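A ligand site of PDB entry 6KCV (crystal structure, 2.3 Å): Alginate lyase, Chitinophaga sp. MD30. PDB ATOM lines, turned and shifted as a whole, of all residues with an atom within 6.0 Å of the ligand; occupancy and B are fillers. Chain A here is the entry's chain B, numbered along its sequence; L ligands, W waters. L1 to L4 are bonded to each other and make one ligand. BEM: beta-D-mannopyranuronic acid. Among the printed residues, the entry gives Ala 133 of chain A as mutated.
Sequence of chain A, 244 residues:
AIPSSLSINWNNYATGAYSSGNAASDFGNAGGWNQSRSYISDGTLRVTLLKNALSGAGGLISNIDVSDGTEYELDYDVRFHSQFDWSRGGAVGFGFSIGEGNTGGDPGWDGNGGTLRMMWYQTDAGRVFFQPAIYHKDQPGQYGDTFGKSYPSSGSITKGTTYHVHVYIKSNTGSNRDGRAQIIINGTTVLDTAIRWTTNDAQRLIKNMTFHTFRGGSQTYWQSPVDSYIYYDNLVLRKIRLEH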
ATOM      1  N   LEU A  54       8.379  -3.641   8.810  1.00  0.00           N
ATOM      2  CA  LEU A  54       8.701  -4.572   9.890  1.00  0.00           C
ATOM      3  C   LEU A  54       9.406  -5.806   9.340  1.00  0.00           C
ATOM      4  O   LEU A  54       9.411  -6.066   8.133  1.00  0.00           O
ATOM      5  CB  LEU A  54       7.428  -5.012  10.634  1.00  0.00           C
ATOM      6  CG  LEU A  54       6.482  -3.924  11.150  1.00  0.00           C
ATOM      7  CD1 LEU A  54       5.177  -4.550  11.597  1.00  0.00           C
ATOM      8  CD2 LEU A  54       7.126  -3.181  12.307  1.00  0.00           C
ATOM      9  N   SER A  55      10.008  -6.560  10.256  1.00  0.00           N
ATOM     10  CA  SER A  55      10.537  -7.923   9.996  1.00  0.00           C
ATOM     11  C   SER A  55      11.544  -7.843   8.850  1.00  0.00           C
ATOM     12  O   SER A  55      12.269  -6.838   8.726  1.00  0.00           O
ATOM     13  CB  SER A  55       9.404  -8.893   9.743  1.00  0.00           C
ATOM     14  OG  SER A  55       8.298  -8.570  10.550  1.00  0.00           O
ATOM     15  N   GLY A  56      11.581  -8.877   7.997  1.00  0.00           N
ATOM     16  CA  GLY A  56      12.532  -8.912   6.899  1.00  0.00           C
ATOM     17  C   GLY A  56      12.286  -7.822   5.871  1.00  0.00           C
ATOM     18  O   GLY A  56      13.224  -7.372   5.217  1.00  0.00           O
ATOM     19  N   ALA A  57      11.025  -7.368   5.756  1.00  0.00           N
ATOM     20  CA  ALA A  57      10.711  -6.303   4.797  1.00  0.00           C
ATOM     21  C   ALA A  57      11.504  -5.035   5.095  1.00  0.00           C
ATOM     22  O   ALA A  57      11.846  -4.304   4.169  1.00  0.00           O
ATOM     23  CB  ALA A  57       9.206  -6.019   4.797  1.00  0.00           C
ATOM     24  N   ILE A  61      17.877  -9.996   8.423  1.00  0.00           N
ATOM     25  CA  ILE A  61      17.629 -11.262   9.105  1.00  0.00           C
ATOM     26  C   ILE A  61      18.528 -12.291   8.442  1.00  0.00           C
ATOM     27  O   ILE A  61      18.195 -12.851   7.395  1.00  0.00           O
ATOM     28  CB  ILE A  61      16.155 -11.673   9.046  1.00  0.00           C
ATOM     29  CG1 ILE A  61      15.272 -10.570   9.659  1.00  0.00           C
ATOM     30  CG2 ILE A  61      15.929 -13.001   9.758  1.00  0.00           C
ATOM     31  CD1 ILE A  61      13.782 -10.893   9.634  1.00  0.00           C
ATOM     32  N   ARG A  88       7.818   0.550  19.358  1.00  0.00           N
ATOM     33  CA  ARG A  88       7.350  -0.498  20.273  1.00  0.00           C
ATOM     34  C   ARG A  88       8.452  -1.496  20.616  1.00  0.00           C
ATOM     35  O   ARG A  88       8.507  -1.990  21.745  1.00  0.00           O
ATOM     36  CB  ARG A  88       6.133  -1.223  19.699  1.00  0.00           C
ATOM     37  CG  ARG A  88       5.529  -2.330  20.596  1.00  0.00           C
ATOM     38  CD  ARG A  88       5.145  -1.836  21.982  1.00  0.00           C
ATOM     39  NE  ARG A  88       3.824  -2.333  22.389  1.00  0.00           N
ATOM     40  CZ  ARG A  88       3.172  -1.941  23.477  1.00  0.00           C
ATOM     41  NH1 ARG A  88       3.716  -1.060  24.320  1.00  0.00           N
ATOM     42  NH2 ARG A  88       1.973  -2.433  23.736  1.00  0.00           N
ATOM     43  N   THR A 103      11.331 -19.867  15.120  1.00  0.00           N
ATOM     44  CA  THR A 103      11.143 -18.445  15.325  1.00  0.00           C
ATOM     45  C   THR A 103       9.770 -18.049  14.793  1.00  0.00           C
ATOM     46  O   THR A 103       9.045 -18.874  14.229  1.00  0.00           O
ATOM     47  CB  THR A 103      12.182 -17.595  14.574  1.00  0.00           C
ATOM     48  OG1 THR A 103      12.029 -17.833  13.160  1.00  0.00           O
ATOM     49  CG2 THR A 103      13.612 -17.888  15.041  1.00  0.00           C
ATOM     50  N   GLY A 104       9.436 -16.775  14.955  1.00  0.00           N
ATOM     51  CA  GLY A 104       8.359 -16.143  14.214  1.00  0.00           C
ATOM     52  C   GLY A 104       6.965 -16.706  14.365  1.00  0.00           C
ATOM     53  O   GLY A 104       6.263 -16.880  13.379  1.00  0.00           O
ATOM     54  N   GLY A 105       6.536 -16.966  15.606  1.00  0.00           N
ATOM     55  CA  GLY A 105       5.223 -17.521  15.887  1.00  0.00           C
ATOM     56  C   GLY A 105       5.086 -19.017  15.656  1.00  0.00           C
ATOM     57  O   GLY A 105       3.960 -19.520  15.664  1.00  0.00           O
ATOM     58  N   ARG A 117      17.468 -15.585  21.261  1.00  0.00           N
ATOM     59  CA  ARG A 117      17.714 -14.253  20.723  1.00  0.00           C
ATOM     60  C   ARG A 117      17.271 -13.224  21.743  1.00  0.00           C
ATOM     61  O   ARG A 117      16.743 -13.556  22.810  1.00  0.00           O
ATOM     62  CB  ARG A 117      16.966 -14.024  19.402  1.00  0.00           C
ATOM     63  CG  ARG A 117      17.394 -14.901  18.251  1.00  0.00           C
ATOM     64  CD  ARG A 117      16.472 -14.691  17.057  1.00  0.00           C
ATOM     65  NE  ARG A 117      15.072 -14.966  17.428  1.00  0.00           N
ATOM     66  CZ  ARG A 117      14.023 -14.659  16.672  1.00  0.00           C
ATOM     67  NH1 ARG A 117      14.210 -14.069  15.495  1.00  0.00           N
ATOM     68  NH2 ARG A 117      12.781 -14.938  17.069  1.00  0.00           N
ATOM     69  N   MET A 119      15.443  -9.115  22.252  1.00  0.00           N
ATOM     70  CA  MET A 119      14.578  -8.060  21.744  1.00  0.00           C
ATOM     71  C   MET A 119      14.765  -6.785  22.549  1.00  0.00           C
ATOM     72  O   MET A 119      15.187  -6.818  23.702  1.00  0.00           O
ATOM     73  CB  MET A 119      13.082  -8.443  21.817  1.00  0.00           C
ATOM     74  CG  MET A 119      12.702  -9.783  21.200  1.00  0.00           C
ATOM     75  SD  MET A 119      12.712  -9.808  19.404  1.00  0.00           S
ATOM     76  CE  MET A 119      11.836 -11.332  19.042  1.00  0.00           C
ATOM     77  N   TYR A 121      12.034  -3.589  23.755  1.00  0.00           N
ATOM     78  CA  TYR A 121      10.597  -3.399  23.922  1.00  0.00           C
ATOM     79  C   TYR A 121      10.352  -2.123  24.706  1.00  0.00           C
ATOM     80  O   TYR A 121      11.114  -1.785  25.610  1.00  0.00           O
ATOM     81  CB  TYR A 121       9.956  -4.586  24.649  1.00  0.00           C
ATOM     82  CG  TYR A 121       8.445  -4.543  24.700  1.00  0.00           C
ATOM     83  CD1 TYR A 121       7.690  -4.900  23.595  1.00  0.00           C
ATOM     84  CD2 TYR A 121       7.789  -4.166  25.865  1.00  0.00           C
ATOM     85  CE1 TYR A 121       6.302  -4.886  23.638  1.00  0.00           C
ATOM     86  CE2 TYR A 121       6.397  -4.141  25.916  1.00  0.00           C
ATOM     87  CZ  TYR A 121       5.659  -4.509  24.799  1.00  0.00           C
ATOM     88  OH  TYR A 121       4.281  -4.484  24.846  1.00  0.00           O
ATOM     89  N   GLN A 131      15.040  -7.705  26.362  1.00  0.00           N
ATOM     90  CA  GLN A 131      14.377  -8.851  26.952  1.00  0.00           C
ATOM     91  C   GLN A 131      14.679 -10.096  26.135  1.00  0.00           C
ATOM     92  O   GLN A 131      14.864 -10.013  24.919  1.00  0.00           O
ATOM     93  CB  GLN A 131      12.853  -8.640  27.060  1.00  0.00           C
ATOM     94  CG  GLN A 131      12.104  -8.634  25.735  1.00  0.00           C
ATOM     95  CD  GLN A 131      10.578  -8.496  25.909  1.00  0.00           C
ATOM     96  OE1 GLN A 131      10.063  -8.337  27.030  1.00  0.00           O
ATOM     97  NE2 GLN A 131       9.851  -8.528  24.789  1.00  0.00           N
ATOM     98  N   ALA A 133      14.037 -13.444  24.006  1.00  0.00           N
ATOM     99  CA  ALA A 133      13.003 -14.016  23.140  1.00  0.00           C
ATOM    100  C   ALA A 133      13.426 -15.451  22.881  1.00  0.00           C
ATOM    101  O   ALA A 133      14.254 -15.713  21.995  1.00  0.00           O
ATOM    102  CB  ALA A 133      12.880 -13.222  21.844  1.00  0.00           C
ATOM    103  N   TYR A 135      12.616 -19.390  22.072  1.00  0.00           N
ATOM    104  CA  TYR A 135      11.739 -20.436  21.568  1.00  0.00           C
ATOM    105  C   TYR A 135      12.272 -21.764  22.072  1.00  0.00           C
ATOM    106  O   TYR A 135      13.467 -22.039  21.947  1.00  0.00           O
ATOM    107  CB  TYR A 135      11.660 -20.422  20.039  1.00  0.00           C
ATOM    108  CG  TYR A 135      10.766 -19.345  19.462  1.00  0.00           C
ATOM    109  CD1 TYR A 135      11.111 -18.001  19.550  1.00  0.00           C
ATOM    110  CD2 TYR A 135       9.575 -19.661  18.813  1.00  0.00           C
ATOM    111  CE1 TYR A 135      10.315 -17.005  19.031  1.00  0.00           C
ATOM    112  CE2 TYR A 135       8.753 -18.665  18.281  1.00  0.00           C
ATOM    113  CZ  TYR A 135       9.139 -17.333  18.406  1.00  0.00           C
ATOM    114  OH  TYR A 135       8.356 -16.323  17.900  1.00  0.00           O
ATOM    115  N   TYR A 143       4.773 -17.132  20.385  1.00  0.00           N
ATOM    116  CA  TYR A 143       5.961 -16.323  20.174  1.00  0.00           C
ATOM    117  C   TYR A 143       6.946 -16.526  21.331  1.00  0.00           C
ATOM    118  O   TYR A 143       6.715 -17.330  22.239  1.00  0.00           O
ATOM    119  CB  TYR A 143       5.568 -14.853  19.983  1.00  0.00           C
ATOM    120  CG  TYR A 143       4.775 -14.610  18.705  1.00  0.00           C
ATOM    121  CD1 TYR A 143       5.422 -14.408  17.494  1.00  0.00           C
ATOM    122  CD2 TYR A 143       3.382 -14.604  18.709  1.00  0.00           C
ATOM    123  CE1 TYR A 143       4.699 -14.187  16.317  1.00  0.00           C
ATOM    124  CE2 TYR A 143       2.655 -14.372  17.540  1.00  0.00           C
ATOM    125  CZ  TYR A 143       3.322 -14.176  16.347  1.00  0.00           C
ATOM    126  OH  TYR A 143       2.619 -13.947  15.183  1.00  0.00           O
ATOM    127  N   GLY A 144       8.056 -15.791  21.295  1.00  0.00           N
ATOM    128  CA  GLY A 144       9.181 -16.082  22.166  1.00  0.00           C
ATOM    129  C   GLY A 144       8.862 -15.909  23.648  1.00  0.00           C
ATOM    130  O   GLY A 144       8.021 -15.113  24.061  1.00  0.00           O
ATOM    131  N   HIS A 212      19.715 -11.152  13.677  1.00  0.00           N
ATOM    132  CA  HIS A 212      18.392 -10.662  13.327  1.00  0.00           C
ATOM    133  C   HIS A 212      18.216  -9.263  13.906  1.00  0.00           C
ATOM    134  O   HIS A 212      18.273  -9.083  15.126  1.00  0.00           O
ATOM    135  CB  HIS A 212      17.306 -11.607  13.838  1.00  0.00           C
ATOM    136  CG  HIS A 212      17.377 -13.000  13.281  1.00  0.00           C
ATOM    137  ND1 HIS A 212      16.479 -13.988  13.620  1.00  0.00           N
ATOM    138  CD2 HIS A 212      18.245 -13.558  12.409  1.00  0.00           C
ATOM    139  CE1 HIS A 212      16.784 -15.102  12.973  1.00  0.00           C
ATOM    140  NE2 HIS A 212      17.856 -14.867  12.229  1.00  0.00           N
ATOM    141  N   PHE A 214      15.416  -6.231  13.406  1.00  0.00           N
ATOM    142  CA  PHE A 214      14.175  -5.787  12.772  1.00  0.00           C
ATOM    143  C   PHE A 214      13.253  -5.174  13.811  1.00  0.00           C
ATOM    144  O   PHE A 214      13.416  -5.397  15.012  1.00  0.00           O
ATOM    145  CB  PHE A 214      13.490  -6.935  12.027  1.00  0.00           C
ATOM    146  CG  PHE A 214      13.094  -8.114  12.883  1.00  0.00           C
ATOM    147  CD1 PHE A 214      11.978  -8.066  13.712  1.00  0.00           C
ATOM    148  CD2 PHE A 214      13.813  -9.304  12.813  1.00  0.00           C
ATOM    149  CE1 PHE A 214      11.598  -9.175  14.473  1.00  0.00           C
ATOM    150  CE2 PHE A 214      13.437 -10.423  13.567  1.00  0.00           C
ATOM    151  CZ  PHE A 214      12.331 -10.349  14.403  1.00  0.00           C
ATOM    152  N   GLY A 216       9.285  -4.885  15.210  1.00  0.00           N
ATOM    153  CA  GLY A 216       8.131  -5.751  15.331  1.00  0.00           C
ATOM    154  C   GLY A 216       8.450  -7.064  16.019  1.00  0.00           C
ATOM    155  O   GLY A 216       9.602  -7.406  16.284  1.00  0.00           O
ATOM    156  N   GLY A 217       7.396  -7.823  16.357  1.00  0.00           N
ATOM    157  CA  GLY A 217       6.015  -7.385  16.176  1.00  0.00           C
ATOM    158  C   GLY A 217       5.476  -7.555  14.763  1.00  0.00           C
ATOM    159  O   GLY A 217       6.234  -7.617  13.802  1.00  0.00           O
ATOM    160  N   SER A 218       4.144  -7.608  14.645  1.00  0.00           N
ATOM    161  CA  SER A 218       3.500  -7.619  13.347  1.00  0.00           C
ATOM    162  C   SER A 218       2.428  -6.532  13.196  1.00  0.00           C
ATOM    163  O   SER A 218       1.887  -6.374  12.098  1.00  0.00           O
ATOM    164  CB  SER A 218       2.873  -9.001  13.065  1.00  0.00           C
ATOM    165  OG  SER A 218       2.070  -9.395  14.164  1.00  0.00           O
ATOM    166  N   GLN A 219       2.121  -5.796  14.252  1.00  0.00           N
ATOM    167  CA  GLN A 219       1.141  -4.720  14.200  1.00  0.00           C
ATOM    168  C   GLN A 219       1.815  -3.405  13.760  1.00  0.00           C
ATOM    169  O   GLN A 219       3.001  -3.176  14.025  1.00  0.00           O
ATOM    170  CB  GLN A 219       0.455  -4.571  15.568  1.00  0.00           C
ATOM    171  CG  GLN A 219      -0.197  -5.868  16.141  1.00  0.00           C
ATOM    172  CD  GLN A 219       0.817  -6.940  16.628  1.00  0.00           C
ATOM    173  OE1 GLN A 219       1.986  -6.641  16.901  1.00  0.00           O
ATOM    174  NE2 GLN A 219       0.364  -8.185  16.695  1.00  0.00           N
ATOM    175  N   TYR A 221       1.789  -0.387  14.661  1.00  0.00           N
ATOM    176  CA  TYR A 221       2.367   0.538  15.623  1.00  0.00           C
ATOM    177  C   TYR A 221       3.786   0.172  16.045  1.00  0.00           C
ATOM    178  O   TYR A 221       4.420   0.951  16.765  1.00  0.00           O
ATOM    179  CB  TYR A 221       1.475   0.663  16.867  1.00  0.00           C
ATOM    180  CG  TYR A 221       1.193  -0.636  17.609  1.00  0.00           C
ATOM    181  CD1 TYR A 221       2.174  -1.281  18.378  1.00  0.00           C
ATOM    182  CD2 TYR A 221      -0.081  -1.213  17.565  1.00  0.00           C
ATOM    183  CE1 TYR A 221       1.894  -2.463  19.068  1.00  0.00           C
ATOM    184  CE2 TYR A 221      -0.368  -2.387  18.254  1.00  0.00           C
ATOM    185  CZ  TYR A 221       0.621  -3.011  18.999  1.00  0.00           C
ATOM    186  OH  TYR A 221       0.329  -4.177  19.675  1.00  0.00           O
ATOM    187  N   TRP A 222       4.309  -0.999  15.657  1.00  0.00           N
ATOM    188  CA  TRP A 222       5.740  -1.262  15.858  1.00  0.00           C
ATOM    189  C   TRP A 222       6.623  -0.554  14.834  1.00  0.00           C
ATOM    190  O   TRP A 222       7.846  -0.574  14.989  1.00  0.00           O
ATOM    191  CB  TRP A 222       6.057  -2.758  15.778  1.00  0.00           C
ATOM    192  CG  TRP A 222       5.434  -3.656  16.818  1.00  0.00           C
ATOM    193  CD1 TRP A 222       4.119  -4.034  16.895  1.00  0.00           C
ATOM    194  CD2 TRP A 222       6.115  -4.359  17.878  1.00  0.00           C
ATOM    195  NE1 TRP A 222       3.938  -4.892  17.959  1.00  0.00           N
ATOM    196  CE2 TRP A 222       5.140  -5.114  18.565  1.00  0.00           C
ATOM    197  CE3 TRP A 222       7.447  -4.405  18.317  1.00  0.00           C
ATOM    198  CZ2 TRP A 222       5.460  -5.913  19.669  1.00  0.00           C
ATOM    199  CZ3 TRP A 222       7.760  -5.212  19.403  1.00  0.00           C
ATOM    200  CH2 TRP A 222       6.779  -5.945  20.070  1.00  0.00           C
HETATM  201  C1  BEM L   1      11.613 -14.814   9.868  1.00  0.00           C
HETATM  202  C2  BEM L   1      11.751 -15.166  11.342  1.00  0.00           C
HETATM  203  O2  BEM L   1      13.117 -15.330  11.671  1.00  0.00           O
HETATM  204  C3  BEM L   1      11.048 -14.131  12.232  1.00  0.00           C
HETATM  205  O3  BEM L   1      11.929 -13.700  13.260  1.00  0.00           O
HETATM  206  C4  BEM L   1      10.242 -12.976  11.578  1.00  0.00           C
HETATM  207  O4  BEM L   1       9.092 -12.614  12.360  1.00  0.00           O
HETATM  208  C5  BEM L   1       9.837 -13.313  10.135  1.00  0.00           C
HETATM  209  O5  BEM L   1      11.116 -13.495   9.538  1.00  0.00           O
HETATM  210  C6  BEM L   1       8.791 -12.486   9.377  1.00  0.00           C
HETATM  211  O6B BEM L   1       9.025 -12.003   8.244  1.00  0.00           O
HETATM  212  O6A BEM L   1       7.666 -12.331   9.944  1.00  0.00           O
HETATM  213  O1  BEM L   1      12.910 -15.001   9.347  1.00  0.00           O
HETATM  214  C1  BEM L   2       8.820 -11.695  13.346  1.00  0.00           C
HETATM  215  C2  BEM L   2       7.345 -11.717  13.379  1.00  0.00           C
HETATM  216  O2  BEM L   2       6.980 -13.075  13.430  1.00  0.00           O
HETATM  217  C3  BEM L   2       7.105 -11.054  14.708  1.00  0.00           C
HETATM  218  O3  BEM L   2       5.732 -10.781  14.838  1.00  0.00           O
HETATM  219  C4  BEM L   2       7.695 -11.773  15.922  1.00  0.00           C
HETATM  220  O4  BEM L   2       7.690 -10.967  17.094  1.00  0.00           O
HETATM  221  C5  BEM L   2       9.115 -12.265  15.735  1.00  0.00           C
HETATM  222  O5  BEM L   2       9.287 -12.575  14.365  1.00  0.00           O
HETATM  223  C6  BEM L   2       9.521 -13.461  16.558  1.00  0.00           C
HETATM  224  O6B BEM L   2      10.329 -14.269  16.047  1.00  0.00           O
HETATM  225  O6A BEM L   2       9.021 -13.626  17.690  1.00  0.00           O
HETATM  226  C1  BEM L   3       6.713 -11.056  18.061  1.00  0.00           C
HETATM  227  C2  BEM L   3       6.994 -10.358  19.365  1.00  0.00           C
HETATM  228  O2  BEM L   3       7.354  -9.035  19.078  1.00  0.00           O
HETATM  229  C3  BEM L   3       5.701 -10.387  20.164  1.00  0.00           C
HETATM  230  O3  BEM L   3       5.798  -9.591  21.305  1.00  0.00           O
HETATM  231  C4  BEM L   3       4.468  -9.973  19.379  1.00  0.00           C
HETATM  232  O4  BEM L   3       3.331 -10.021  20.223  1.00  0.00           O
HETATM  233  C5  BEM L   3       4.283 -10.800  18.110  1.00  0.00           C
HETATM  234  O5  BEM L   3       5.491 -10.651  17.403  1.00  0.00           O
HETATM  235  C6  BEM L   3       3.134 -10.433  17.225  1.00  0.00           C
HETATM  236  O6B BEM L   3       3.415 -10.019  16.082  1.00  0.00           O
HETATM  237  O6A BEM L   3       1.969 -10.536  17.678  1.00  0.00           O
HETATM  238  C1  BEM L   4       2.287  -9.126  20.308  1.00  0.00           C
HETATM  239  C2  BEM L   4       1.039  -9.740  20.901  1.00  0.00           C
HETATM  240  O2  BEM L   4       1.384 -10.279  22.167  1.00  0.00           O
HETATM  241  C3  BEM L   4       0.053  -8.612  21.092  1.00  0.00           C
HETATM  242  O3  BEM L   4      -1.089  -9.107  21.745  1.00  0.00           O
HETATM  243  C4  BEM L   4       0.605  -7.416  21.839  1.00  0.00           C
HETATM  244  O4  BEM L   4      -0.361  -6.361  21.940  1.00  0.00           O
HETATM  245  C5  BEM L   4       1.887  -6.918  21.181  1.00  0.00           C
HETATM  246  O5  BEM L   4       2.783  -8.007  21.050  1.00  0.00           O
HETATM  247  C6  BEM L   4       2.471  -5.707  21.841  1.00  0.00           C
HETATM  248  O6B BEM L   4       3.193  -5.836  22.851  1.00  0.00           O
HETATM  249  O6A BEM L   4       2.166  -4.622  21.307  1.00  0.00           O
HETATM  250  O   HOH W   1       9.010 -13.562  20.146  1.00  0.00           O
HETATM  251  O   HOH W   2      -0.877  -9.670  24.263  1.00  0.00           O
HETATM  252  O   HOH W   3       8.951 -11.316  22.101  1.00  0.00           O
HETATM  253  O   HOH W   4       3.855  -9.123  23.409  1.00  0.00           O
HETATM  254  O   HOH W   5       9.848  -8.279  18.938  1.00  0.00           O
HETATM  255  O   HOH W   6      12.586 -13.595   6.874  1.00  0.00           O
HETATM  256  O   HOH W   7       0.183 -12.008  16.016  1.00  0.00           O
HETATM  257  O   HOH W   8       7.959  -8.586  22.687  1.00  0.00           O
HETATM  258  O   HOH W   9      -1.790  -6.604  24.339  1.00  0.00           O
HETATM  259  O   HOH W  10       4.038 -12.635  13.267  1.00  0.00           O
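OH of Tyr 121 sits at hydrogen-bond distance from O6B of BEM L4 (2.6 Å).
NE of Arg 88 lies within salt-bridge range of O6A of BEM L4, at 3.0 Å.
An oxygen (O3) of BEM L2 lies close to the backbone carbonyl oxygen of Gly 217 (3.4 Å).
The guanidinium group (NH2) of Arg 117 is in salt-bridge range of an oxygen (O6B) of BEM L2 (2.7 Å).
An oxygen (O6A) of BEM L2 is in hydrogen-bond range of the side-chain hydroxyl (OH) of Tyr 135, at 2.8 Å.
The backbone NH (N) of Gly 217 sits at hydrogen-bond distance from an oxygen (O2) of BEM L3, 3.0 Å away.
O2 of BEM L1 is in hydrogen-bond range of OG1 of Thr 103 (3.1 Å).
O6B of BEM L3 sits at hydrogen-bond distance from OG of Ser 218, at 2.4 Å.
N of Gly 104 is in hydrogen-bond range of O6B of BEM L2, 2.9 Å away.
NE2 of Gln 219 is in hydrogen-bond range of O6A of BEM L3 (3.0 Å).
N of Ser 218 lies within hydrogen-bond range of O6B of BEM L3 (2.9 Å).
The side-chain hydroxyl (OH) of Tyr 221 is in hydrogen-bond range of an oxygen (O6A) of BEM L4.
The guanidinium group (NH1) of Arg 117 lies within hydrogen-bond range of a ring nitrogen (ND1) of His 212 (2.9 Å).
The guanidinium group (NH2) of Arg 88 sits close to the side-chain hydroxyl (OH) of Tyr 121 (3.3 Å).
The backbone NH (N) of Gln 131 is in hydrogen-bond range of the backbone carbonyl oxygen (O) of Met 119, at 2.8 Å.
OH of Tyr 135 is in hydrogen-bond range of N of Gly 105 (3.0 Å).
The indole nitrogen (NE1) of Trp 222 is in hydrogen-bond range of the side-chain amide oxygen (OE1) of Gln 219.
NE2 of Gln 219 is in hydrogen-bond range of OG of Ser 218 (3.3 Å).
The side-chain hydroxyl of Tyr 135 lies close to the backbone NH of Gly 144, at 3.4 Å.
The side-chain hydroxyl (OH) of Tyr 135 lies within hydrogen-bond range of the backbone NH (N) of Gly 104, 3.2 Å away.
Residues that only touch the ligand: Trp 222 (3.3 Å), Ser 55 (3.5 Å), Phe 214 (3.6 Å), Tyr 143 (3.6 Å), Ile 61 (3.6 Å), Gly 216 (3.8 Å), Met 119 (3.9 Å) and His 212 (3.9 Å).
Hydrophobic or aromatic side chains within 4 Å of the ligand: Ile 61, Met 119, Tyr 121, Tyr 135, Tyr 143, His 212, Phe 214, Tyr 221 and Trp 222.
18 residues have an atom within 4 Å of the ligand: Ser 55, Ile 61, Arg 88, Thr 103, Gly 104, Arg 117, Met 119, Tyr 121, Tyr 135, Tyr 143, His 212, Phe 214, Gly 216, Gly 217, Ser 218, Gln 219, Tyr 221 and Trp 222.
The nearest printed residue that does not touch the ligand is Gly 56 (4.05 Å).
Water W1 lies within hydrogen-bond range of O6A of BEM L2 and N of Gly 144.
Water W5 lies within hydrogen-bond range of an oxygen (O2) of BEM L3 (2.6 Å), the backbone carbonyl oxygen of Gly 216 (2.8 Å) and the side-chain sulfur of Met 119 (3.3 Å).
Water W8 bridges O3 of BEM L3 and NE2 of Gln 131.
Water W7 bridges O6A of BEM L3 (2.8 Å) and OH of Tyr 143 (3.2 Å).
Water W10 bridges OH of Tyr 143 (2.7 Å) and O3 of BEM L2 (3.0 Å).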
